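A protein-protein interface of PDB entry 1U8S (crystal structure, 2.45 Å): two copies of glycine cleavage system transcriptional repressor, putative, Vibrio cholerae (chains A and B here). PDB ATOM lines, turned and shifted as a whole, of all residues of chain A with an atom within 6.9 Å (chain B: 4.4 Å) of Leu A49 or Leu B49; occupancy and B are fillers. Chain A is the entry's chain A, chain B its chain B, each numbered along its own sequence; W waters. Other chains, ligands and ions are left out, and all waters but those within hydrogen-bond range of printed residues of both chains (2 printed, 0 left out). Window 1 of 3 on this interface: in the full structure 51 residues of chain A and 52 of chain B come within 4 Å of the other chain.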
ATOM      1  N   VAL A   8     -36.069  21.829 -24.899  1.00  0.00           N
ATOM      2  CA  VAL A   8     -35.029  22.749 -24.471  1.00  0.00           C
ATOM      3  C   VAL A   8     -35.726  24.042 -24.086  1.00  0.00           C
ATOM      4  O   VAL A   8     -36.471  24.615 -24.876  1.00  0.00           O
ATOM      5  CB  VAL A   8     -34.041  23.038 -25.612  1.00  0.00           C
ATOM      6  CG1 VAL A   8     -33.138  24.203 -25.240  1.00  0.00           C
ATOM      7  CG2 VAL A   8     -33.216  21.785 -25.916  1.00  0.00           C
ATOM      8  N   ILE A   9     -35.500  24.498 -22.869  1.00  0.00           N
ATOM      9  CA  ILE A   9     -36.129  25.717 -22.408  1.00  0.00           C
ATOM     10  C   ILE A   9     -35.066  26.743 -22.101  1.00  0.00           C
ATOM     11  O   ILE A   9     -33.990  26.410 -21.600  1.00  0.00           O
ATOM     12  CB  ILE A   9     -36.936  25.465 -21.122  1.00  0.00           C
ATOM     13  CG1 ILE A   9     -38.107  24.522 -21.419  1.00  0.00           C
ATOM     14  CG2 ILE A   9     -37.418  26.781 -20.532  1.00  0.00           C
ATOM     15  CD1 ILE A   9     -38.840  24.060 -20.172  1.00  0.00           C
ATOM     16  N   THR A  10     -35.353  27.998 -22.403  1.00  0.00           N
ATOM     17  CA  THR A  10     -34.402  29.042 -22.098  1.00  0.00           C
ATOM     18  C   THR A  10     -35.180  30.240 -21.598  1.00  0.00           C
ATOM     19  O   THR A  10     -36.181  30.627 -22.198  1.00  0.00           O
ATOM     20  CB  THR A  10     -33.580  29.416 -23.320  1.00  0.00           C
ATOM     21  OG1 THR A  10     -32.678  30.463 -22.967  1.00  0.00           O
ATOM     22  CG2 THR A  10     -34.459  29.889 -24.439  1.00  0.00           C
ATOM     23  N   ALA A  11     -34.742  30.812 -20.484  1.00  0.00           N
ATOM     24  CA  ALA A  11     -35.431  31.959 -19.921  1.00  0.00           C
ATOM     25  C   ALA A  11     -34.461  33.024 -19.446  1.00  0.00           C
ATOM     26  O   ALA A  11     -33.307  32.732 -19.152  1.00  0.00           O
ATOM     27  CB  ALA A  11     -36.328  31.512 -18.773  1.00  0.00           C
ATOM     28  N   VAL A  12     -34.936  34.264 -19.399  1.00  0.00           N
ATOM     29  CA  VAL A  12     -34.138  35.402 -18.951  1.00  0.00           C
ATOM     30  C   VAL A  12     -35.091  36.435 -18.381  1.00  0.00           C
ATOM     31  O   VAL A  12     -35.900  37.014 -19.108  1.00  0.00           O
ATOM     32  CB  VAL A  12     -33.374  36.072 -20.100  1.00  0.00           C
ATOM     33  CG1 VAL A  12     -32.525  37.202 -19.562  1.00  0.00           C
ATOM     34  CG2 VAL A  12     -32.504  35.068 -20.801  1.00  0.00           C
ATOM     35  N   ASP A  36     -31.030  18.176 -17.244  1.00  0.00           N
ATOM     36  CA  ASP A  36     -29.856  19.004 -17.023  1.00  0.00           C
ATOM     37  C   ASP A  36     -30.300  20.458 -17.181  1.00  0.00           C
ATOM     38  O   ASP A  36     -31.424  20.728 -17.609  1.00  0.00           O
ATOM     39  CB  ASP A  36     -28.783  18.646 -18.054  1.00  0.00           C
ATOM     40  CG  ASP A  36     -27.387  19.033 -17.612  1.00  0.00           C
ATOM     41  OD1 ASP A  36     -27.211  19.449 -16.450  1.00  0.00           O
ATOM     42  OD2 ASP A  36     -26.455  18.903 -18.433  1.00  0.00           O
ATOM     43  N   SER A  37     -29.427  21.388 -16.822  1.00  0.00           N
ATOM     44  CA  SER A  37     -29.758  22.794 -16.937  1.00  0.00           C
ATOM     45  C   SER A  37     -28.526  23.624 -16.600  1.00  0.00           C
ATOM     46  O   SER A  37     -27.547  23.107 -16.075  1.00  0.00           O
ATOM     47  CB  SER A  37     -30.912  23.157 -15.978  1.00  0.00           C
ATOM     48  OG  SER A  37     -30.532  23.029 -14.612  1.00  0.00           O
ATOM     49  N   ARG A  38     -28.567  24.905 -16.940  1.00  0.00           N
ATOM     50  CA  ARG A  38     -27.469  25.813 -16.631  1.00  0.00           C
ATOM     51  C   ARG A  38     -28.152  27.036 -16.065  1.00  0.00           C
ATOM     52  O   ARG A  38     -29.116  27.559 -16.650  1.00  0.00           O
ATOM     53  CB  ARG A  38     -26.676  26.190 -17.884  1.00  0.00           C
ATOM     54  CG  ARG A  38     -25.864  25.061 -18.422  1.00  0.00           C
ATOM     55  CD  ARG A  38     -24.901  24.513 -17.369  1.00  0.00           C
ATOM     56  NE  ARG A  38     -24.047  23.497 -17.981  1.00  0.00           N
ATOM     57  CZ  ARG A  38     -24.375  22.220 -18.139  1.00  0.00           C
ATOM     58  NH1 ARG A  38     -25.544  21.756 -17.707  1.00  0.00           N
ATOM     59  NH2 ARG A  38     -23.560  21.421 -18.816  1.00  0.00           N
ATOM     60  N   ILE A  39     -27.681  27.458 -14.904  1.00  0.00           N
ATOM     61  CA  ILE A  39     -28.251  28.605 -14.249  1.00  0.00           C
ATOM     62  C   ILE A  39     -27.151  29.610 -13.996  1.00  0.00           C
ATOM     63  O   ILE A  39     -26.036  29.249 -13.620  1.00  0.00           O
ATOM     64  CB  ILE A  39     -28.886  28.190 -12.924  1.00  0.00           C
ATOM     65  CG1 ILE A  39     -29.833  27.015 -13.168  1.00  0.00           C
ATOM     66  CG2 ILE A  39     -29.605  29.377 -12.288  1.00  0.00           C
ATOM     67  CD1 ILE A  39     -30.558  26.527 -11.916  1.00  0.00           C
ATOM     68  N   ALA A  40     -27.456  30.875 -14.218  1.00  0.00           N
ATOM     69  CA  ALA A  40     -26.460  31.903 -13.999  1.00  0.00           C
ATOM     70  C   ALA A  40     -27.147  33.223 -13.718  1.00  0.00           C
ATOM     71  O   ALA A  40     -28.268  33.469 -14.165  1.00  0.00           O
ATOM     72  CB  ALA A  40     -25.561  32.025 -15.231  1.00  0.00           C
ATOM     73  N   PHE A  42     -26.514  36.840 -14.516  1.00  0.00           N
ATOM     74  CA  PHE A  42     -25.716  37.773 -15.298  1.00  0.00           C
ATOM     75  C   PHE A  42     -26.231  39.182 -15.124  1.00  0.00           C
ATOM     76  O   PHE A  42     -27.406  39.453 -15.372  1.00  0.00           O
ATOM     77  CB  PHE A  42     -25.752  37.420 -16.791  1.00  0.00           C
ATOM     78  CG  PHE A  42     -25.017  36.155 -17.145  1.00  0.00           C
ATOM     79  CD1 PHE A  42     -23.954  35.708 -16.366  1.00  0.00           C
ATOM     80  CD2 PHE A  42     -25.348  35.440 -18.291  1.00  0.00           C
ATOM     81  CE1 PHE A  42     -23.233  34.575 -16.719  1.00  0.00           C
ATOM     82  CE2 PHE A  42     -24.628  34.305 -18.651  1.00  0.00           C
ATOM     83  CZ  PHE A  42     -23.567  33.876 -17.859  1.00  0.00           C
ATOM     84  N   PHE A  46     -31.856  36.751 -14.073  1.00  0.00           N
ATOM     85  CA  PHE A  46     -31.836  35.322 -13.788  1.00  0.00           C
ATOM     86  C   PHE A  46     -31.696  34.727 -15.195  1.00  0.00           C
ATOM     87  O   PHE A  46     -32.388  35.163 -16.111  1.00  0.00           O
ATOM     88  CB  PHE A  46     -33.161  34.887 -13.178  1.00  0.00           C
ATOM     89  CG  PHE A  46     -33.424  33.414 -13.291  1.00  0.00           C
ATOM     90  CD1 PHE A  46     -32.769  32.512 -12.461  1.00  0.00           C
ATOM     91  CD2 PHE A  46     -34.322  32.925 -14.239  1.00  0.00           C
ATOM     92  CE1 PHE A  46     -33.001  31.138 -12.567  1.00  0.00           C
ATOM     93  CE2 PHE A  46     -34.562  31.549 -14.356  1.00  0.00           C
ATOM     94  CZ  PHE A  46     -33.898  30.658 -13.515  1.00  0.00           C
ATOM     95  N   THR A  47     -30.811  33.750 -15.367  1.00  0.00           N
ATOM     96  CA  THR A  47     -30.589  33.146 -16.678  1.00  0.00           C
ATOM     97  C   THR A  47     -30.698  31.623 -16.655  1.00  0.00           C
ATOM     98  O   THR A  47     -30.040  30.960 -15.854  1.00  0.00           O
ATOM     99  CB  THR A  47     -29.206  33.544 -17.208  1.00  0.00           C
ATOM    100  OG1 THR A  47     -29.088  34.974 -17.220  1.00  0.00           O
ATOM    101  CG2 THR A  47     -29.029  33.062 -18.604  1.00  0.00           C
ATOM    102  N   LEU A  48     -31.504  31.058 -17.554  1.00  0.00           N
ATOM    103  CA  LEU A  48     -31.675  29.610 -17.559  1.00  0.00           C
ATOM    104  C   LEU A  48     -31.646  28.836 -18.878  1.00  0.00           C
ATOM    105  O   LEU A  48     -32.264  29.217 -19.868  1.00  0.00           O
ATOM    106  CB  LEU A  48     -32.978  29.246 -16.834  1.00  0.00           C
ATOM    107  CG  LEU A  48     -33.368  27.758 -16.820  1.00  0.00           C
ATOM    108  CD1 LEU A  48     -32.434  26.980 -15.903  1.00  0.00           C
ATOM    109  CD2 LEU A  48     -34.814  27.612 -16.342  1.00  0.00           C
ATOM    110  N   LEU A  49     -30.918  27.729 -18.859  1.00  0.00           N
ATOM    111  CA  LEU A  49     -30.861  26.818 -19.984  1.00  0.00           C
ATOM    112  C   LEU A  49     -31.324  25.542 -19.314  1.00  0.00           C
ATOM    113  O   LEU A  49     -30.799  25.185 -18.264  1.00  0.00           O
ATOM    114  CB  LEU A  49     -29.438  26.628 -20.496  1.00  0.00           C
ATOM    115  CG  LEU A  49     -28.809  27.783 -21.271  1.00  0.00           C
ATOM    116  CD1 LEU A  49     -27.392  27.397 -21.693  1.00  0.00           C
ATOM    117  CD2 LEU A  49     -29.666  28.113 -22.484  1.00  0.00           C
ATOM    118  N   MET A  50     -32.302  24.861 -19.898  1.00  0.00           N
ATOM    119  CA  MET A  50     -32.807  23.647 -19.299  1.00  0.00           C
ATOM    120  C   MET A  50     -33.309  22.675 -20.345  1.00  0.00           C
ATOM    121  O   MET A  50     -33.951  23.066 -21.326  1.00  0.00           O
ATOM    122  CB  MET A  50     -33.933  23.984 -18.318  1.00  0.00           C
ATOM    123  CG  MET A  50     -34.593  22.787 -17.641  1.00  0.00           C
ATOM    124  SD  MET A  50     -35.821  23.340 -16.434  1.00  0.00           S
ATOM    125  CE  MET A  50     -34.756  24.047 -15.191  1.00  0.00           C
ATOM    126  N   LEU A  51     -32.986  21.403 -20.133  1.00  0.00           N
ATOM    127  CA  LEU A  51     -33.404  20.326 -21.014  1.00  0.00           C
ATOM    128  C   LEU A  51     -34.266  19.394 -20.176  1.00  0.00           C
ATOM    129  O   LEU A  51     -33.779  18.768 -19.234  1.00  0.00           O
ATOM    130  CB  LEU A  51     -32.199  19.553 -21.559  1.00  0.00           C
ATOM    131  CG  LEU A  51     -32.616  18.182 -22.110  1.00  0.00           C
ATOM    132  CD1 LEU A  51     -33.345  18.368 -23.453  1.00  0.00           C
ATOM    133  CD2 LEU A  51     -31.411  17.290 -22.291  1.00  0.00           C
ATOM    134  N   LEU A 124     -17.072  30.664 -21.691  1.00  0.00           N
ATOM    135  CA  LEU A 124     -16.161  31.514 -22.446  1.00  0.00           C
ATOM    136  C   LEU A 124     -16.302  32.978 -22.091  1.00  0.00           C
ATOM    137  O   LEU A 124     -17.413  33.505 -22.033  1.00  0.00           O
ATOM    138  CB  LEU A 124     -16.434  31.379 -23.953  1.00  0.00           C
ATOM    139  CG  LEU A 124     -15.802  32.432 -24.880  1.00  0.00           C
ATOM    140  CD1 LEU A 124     -14.355  32.122 -25.043  1.00  0.00           C
ATOM    141  CD2 LEU A 124     -16.449  32.411 -26.257  1.00  0.00           C
ATOM    142  N   ILE B   9     -27.630  37.513 -23.737  1.00  0.00           N
ATOM    143  CA  ILE B   9     -28.047  36.775 -24.916  1.00  0.00           C
ATOM    144  C   ILE B   9     -28.390  35.310 -24.646  1.00  0.00           C
ATOM    145  O   ILE B   9     -27.715  34.619 -23.882  1.00  0.00           O
ATOM    146  CB  ILE B   9     -26.960  36.825 -26.010  1.00  0.00           C
ATOM    147  CG1 ILE B   9     -26.731  38.270 -26.458  1.00  0.00           C
ATOM    148  CG2 ILE B   9     -27.381  35.976 -27.203  1.00  0.00           C
ATOM    149  CD1 ILE B   9     -25.556  38.427 -27.423  1.00  0.00           C
ATOM    150  N   THR B  10     -29.455  34.856 -25.292  1.00  0.00           N
ATOM    151  CA  THR B  10     -29.912  33.489 -25.185  1.00  0.00           C
ATOM    152  C   THR B  10     -30.058  32.971 -26.608  1.00  0.00           C
ATOM    153  O   THR B  10     -30.610  33.653 -27.466  1.00  0.00           O
ATOM    154  CB  THR B  10     -31.272  33.409 -24.466  1.00  0.00           C
ATOM    155  OG1 THR B  10     -31.060  33.083 -23.087  1.00  0.00           O
ATOM    156  CG2 THR B  10     -32.154  32.356 -25.101  1.00  0.00           C
ATOM    157  N   SER B  37     -20.189  33.336 -20.102  1.00  0.00           N
ATOM    158  CA  SER B  37     -21.148  32.594 -20.902  1.00  0.00           C
ATOM    159  C   SER B  37     -21.250  31.167 -20.423  1.00  0.00           C
ATOM    160  O   SER B  37     -20.440  30.711 -19.618  1.00  0.00           O
ATOM    161  CB  SER B  37     -20.724  32.579 -22.375  1.00  0.00           C
ATOM    162  OG  SER B  37     -19.500  31.891 -22.545  1.00  0.00           O
ATOM    163  N   ARG B  38     -22.257  30.469 -20.930  1.00  0.00           N
ATOM    164  CA  ARG B  38     -22.475  29.069 -20.609  1.00  0.00           C
ATOM    165  C   ARG B  38     -22.886  28.401 -21.911  1.00  0.00           C
ATOM    166  O   ARG B  38     -23.790  28.867 -22.628  1.00  0.00           O
ATOM    167  CB  ARG B  38     -23.579  28.906 -19.573  1.00  0.00           C
ATOM    168  CG  ARG B  38     -23.263  29.539 -18.238  1.00  0.00           C
ATOM    169  CD  ARG B  38     -22.241  28.751 -17.451  1.00  0.00           C
ATOM    170  NE  ARG B  38     -22.194  29.263 -16.091  1.00  0.00           N
ATOM    171  CZ  ARG B  38     -21.572  30.384 -15.743  1.00  0.00           C
ATOM    172  NH1 ARG B  38     -20.920  31.100 -16.663  1.00  0.00           N
ATOM    173  NH2 ARG B  38     -21.645  30.815 -14.489  1.00  0.00           N
ATOM    174  N   PHE B  42     -27.543  20.214 -25.484  1.00  0.00           N
ATOM    175  CA  PHE B  42     -28.713  19.470 -25.004  1.00  0.00           C
ATOM    176  C   PHE B  42     -29.421  18.838 -26.181  1.00  0.00           C
ATOM    177  O   PHE B  42     -29.885  19.543 -27.086  1.00  0.00           O
ATOM    178  CB  PHE B  42     -29.706  20.386 -24.292  1.00  0.00           C
ATOM    179  CG  PHE B  42     -29.207  20.926 -22.999  1.00  0.00           C
ATOM    180  CD1 PHE B  42     -28.098  20.360 -22.376  1.00  0.00           C
ATOM    181  CD2 PHE B  42     -29.870  21.972 -22.369  1.00  0.00           C
ATOM    182  CE1 PHE B  42     -27.661  20.828 -21.147  1.00  0.00           C
ATOM    183  CE2 PHE B  42     -29.441  22.449 -21.136  1.00  0.00           C
ATOM    184  CZ  PHE B  42     -28.335  21.874 -20.526  1.00  0.00           C
ATOM    185  N   THR B  47     -26.960  25.174 -27.021  1.00  0.00           N
ATOM    186  CA  THR B  47     -27.602  26.163 -26.156  1.00  0.00           C
ATOM    187  C   THR B  47     -26.547  27.070 -25.550  1.00  0.00           C
ATOM    188  O   THR B  47     -25.515  26.597 -25.054  1.00  0.00           O
ATOM    189  CB  THR B  47     -28.439  25.507 -25.015  1.00  0.00           C
ATOM    190  OG1 THR B  47     -27.583  24.750 -24.161  1.00  0.00           O
ATOM    191  CG2 THR B  47     -29.483  24.580 -25.587  1.00  0.00           C
ATOM    192  N   LEU B  48     -26.829  28.369 -25.571  1.00  0.00           N
ATOM    193  CA  LEU B  48     -25.905  29.379 -25.069  1.00  0.00           C
ATOM    194  C   LEU B  48     -26.491  30.512 -24.203  1.00  0.00           C
ATOM    195  O   LEU B  48     -27.487  31.140 -24.566  1.00  0.00           O
ATOM    196  CB  LEU B  48     -25.199  30.001 -26.264  1.00  0.00           C
ATOM    197  CG  LEU B  48     -24.463  31.300 -26.019  1.00  0.00           C
ATOM    198  CD1 LEU B  48     -23.056  30.987 -25.599  1.00  0.00           C
ATOM    199  CD2 LEU B  48     -24.452  32.122 -27.296  1.00  0.00           C
ATOM    200  N   LEU B  49     -25.859  30.761 -23.056  1.00  0.00           N
ATOM    201  CA  LEU B  49     -26.248  31.867 -22.183  1.00  0.00           C
ATOM    202  C   LEU B  49     -25.068  32.792 -22.318  1.00  0.00           C
ATOM    203  O   LEU B  49     -23.937  32.332 -22.244  1.00  0.00           O
ATOM    204  CB  LEU B  49     -26.364  31.434 -20.723  1.00  0.00           C
ATOM    205  CG  LEU B  49     -27.514  30.478 -20.432  1.00  0.00           C
ATOM    206  CD1 LEU B  49     -27.631  30.242 -18.925  1.00  0.00           C
ATOM    207  CD2 LEU B  49     -28.816  31.064 -21.019  1.00  0.00           C
ATOM    208  N   MET B  50     -25.301  34.079 -22.531  1.00  0.00           N
ATOM    209  CA  MET B  50     -24.160  34.971 -22.668  1.00  0.00           C
ATOM    210  C   MET B  50     -24.440  36.392 -22.209  1.00  0.00           C
ATOM    211  O   MET B  50     -25.558  36.883 -22.318  1.00  0.00           O
ATOM    212  CB  MET B  50     -23.662  34.971 -24.117  1.00  0.00           C
ATOM    213  CG  MET B  50     -22.362  35.712 -24.331  1.00  0.00           C
ATOM    214  SD  MET B  50     -21.829  35.691 -26.070  1.00  0.00           S
ATOM    215  CE  MET B  50     -20.896  34.140 -26.142  1.00  0.00           C
HETATM  216  O   HOH W   1     -24.118  27.619 -15.285  1.00  0.00           O
HETATM  217  O   HOH W   2     -23.531  30.128 -12.315  1.00  0.00           O
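Water W1 bridges the guanidinium group of Arg B38 (2.7 Å) and the backbone carbonyl oxygen of Ile A39 (3.0 Å).
Water W2 lies within hydrogen-bond range of O of Ile A39 (3.0 Å) and NH2 of Arg B38 (3.0 Å).
Of the printed residues of chain A, Thr B10 touches Thr A10 (2.9 Å) and Val A12 (3.4 Å).
Of the printed residues of chain A, Ser B37 touches Leu A124.
Arg B38 touches none of the printed residues of chain A.
Leu B48 touches none of the printed residues of chain A.
Printed residues of chain A within 4 Å of Leu B49: Arg A38 (3.8 Å), Phe A42 (3.9 Å), Thr A47 (3.1 Å) and Leu A49 (3.1 Å).
The nearest printed residue of chain A that does not touch Met B50 is Leu A124 (4.8 Å).
Hydrophobic or aromatic side chains of chain B within 4 Å of the printed part of chain A: Phe B42 and Leu B49.
Among the printed residues, 15 pairs touch across the chains.
Among the printed residues, no Asp or Glu carboxylate lies within 4 Å of a Lys or Arg side-chain nitrogen of the other chain.
Arg A38 touches Leu B49, but with the chains exchanged Leu A49 does not touch Arg B38 (4.001 Å).
Phe A42 touches Met B50, and with the chains exchanged Met A50 touches Phe B42.
Thr A47 touches Leu B49, and with the chains exchanged Leu A49 touches Thr B47.
Leu A49 touches its own counterpart, Leu B49.
Among the printed residues, merely in contact across the chains: Val A8 with Thr B47 (3.7 Å), Val A12 with Thr B10 (3.4 Å), Asp A36 with Phe B42 (3.5 Å), Ser A37 with Phe B42 (3.9 Å), Arg A38 with Phe B42 (3.97 Å), Arg A38 with Leu B49 (3.8 Å), Phe A42 with Leu B49 (3.9 Å), Phe A42 with Met B50 (3.9 Å), Thr A47 with Leu B49 (3.1 Å), Leu A49 with Thr B47 (3.6 Å), Leu A49 with Leu B49 (3.1 Å), Met A50 with Phe B42 (3.9 Å) and Leu A51 with Phe B42 (3.5 Å).
The side-chain hydroxyl (OG1) of Thr B10 lies close to the side-chain hydroxyl (OG1) of Thr A10 (3.1 Å).
The backbone carbonyl oxygen (O) of Leu A124 lies within hydrogen-bond range of the side-chain hydroxyl (OG) of Ser B37 (2.7 Å).
The backbone NH (N) of Ile A9 lies within hydrogen-bond range of the backbone carbonyl oxygen (O) of Met A50 (2.6 Å).
The guanidinium group (NH1) of Arg A38 is in salt-bridge range of the side-chain carboxylate (OD2) of Asp A36.
The backbone carbonyl oxygen (O) of Asp A36 is in hydrogen-bond range of the backbone NH (N) of Leu A51.
The backbone carbonyl oxygen (O) of Leu A49 sits at hydrogen-bond distance from the backbone NH (N) of Arg A38, 2.6 Å away.
The backbone carbonyl oxygen of Ala A40 is in hydrogen-bond range of the backbone NH of Thr A47 (2.8 Å).
O of Met B50 is in hydrogen-bond range of N of Ile B9 (2.6 Å).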
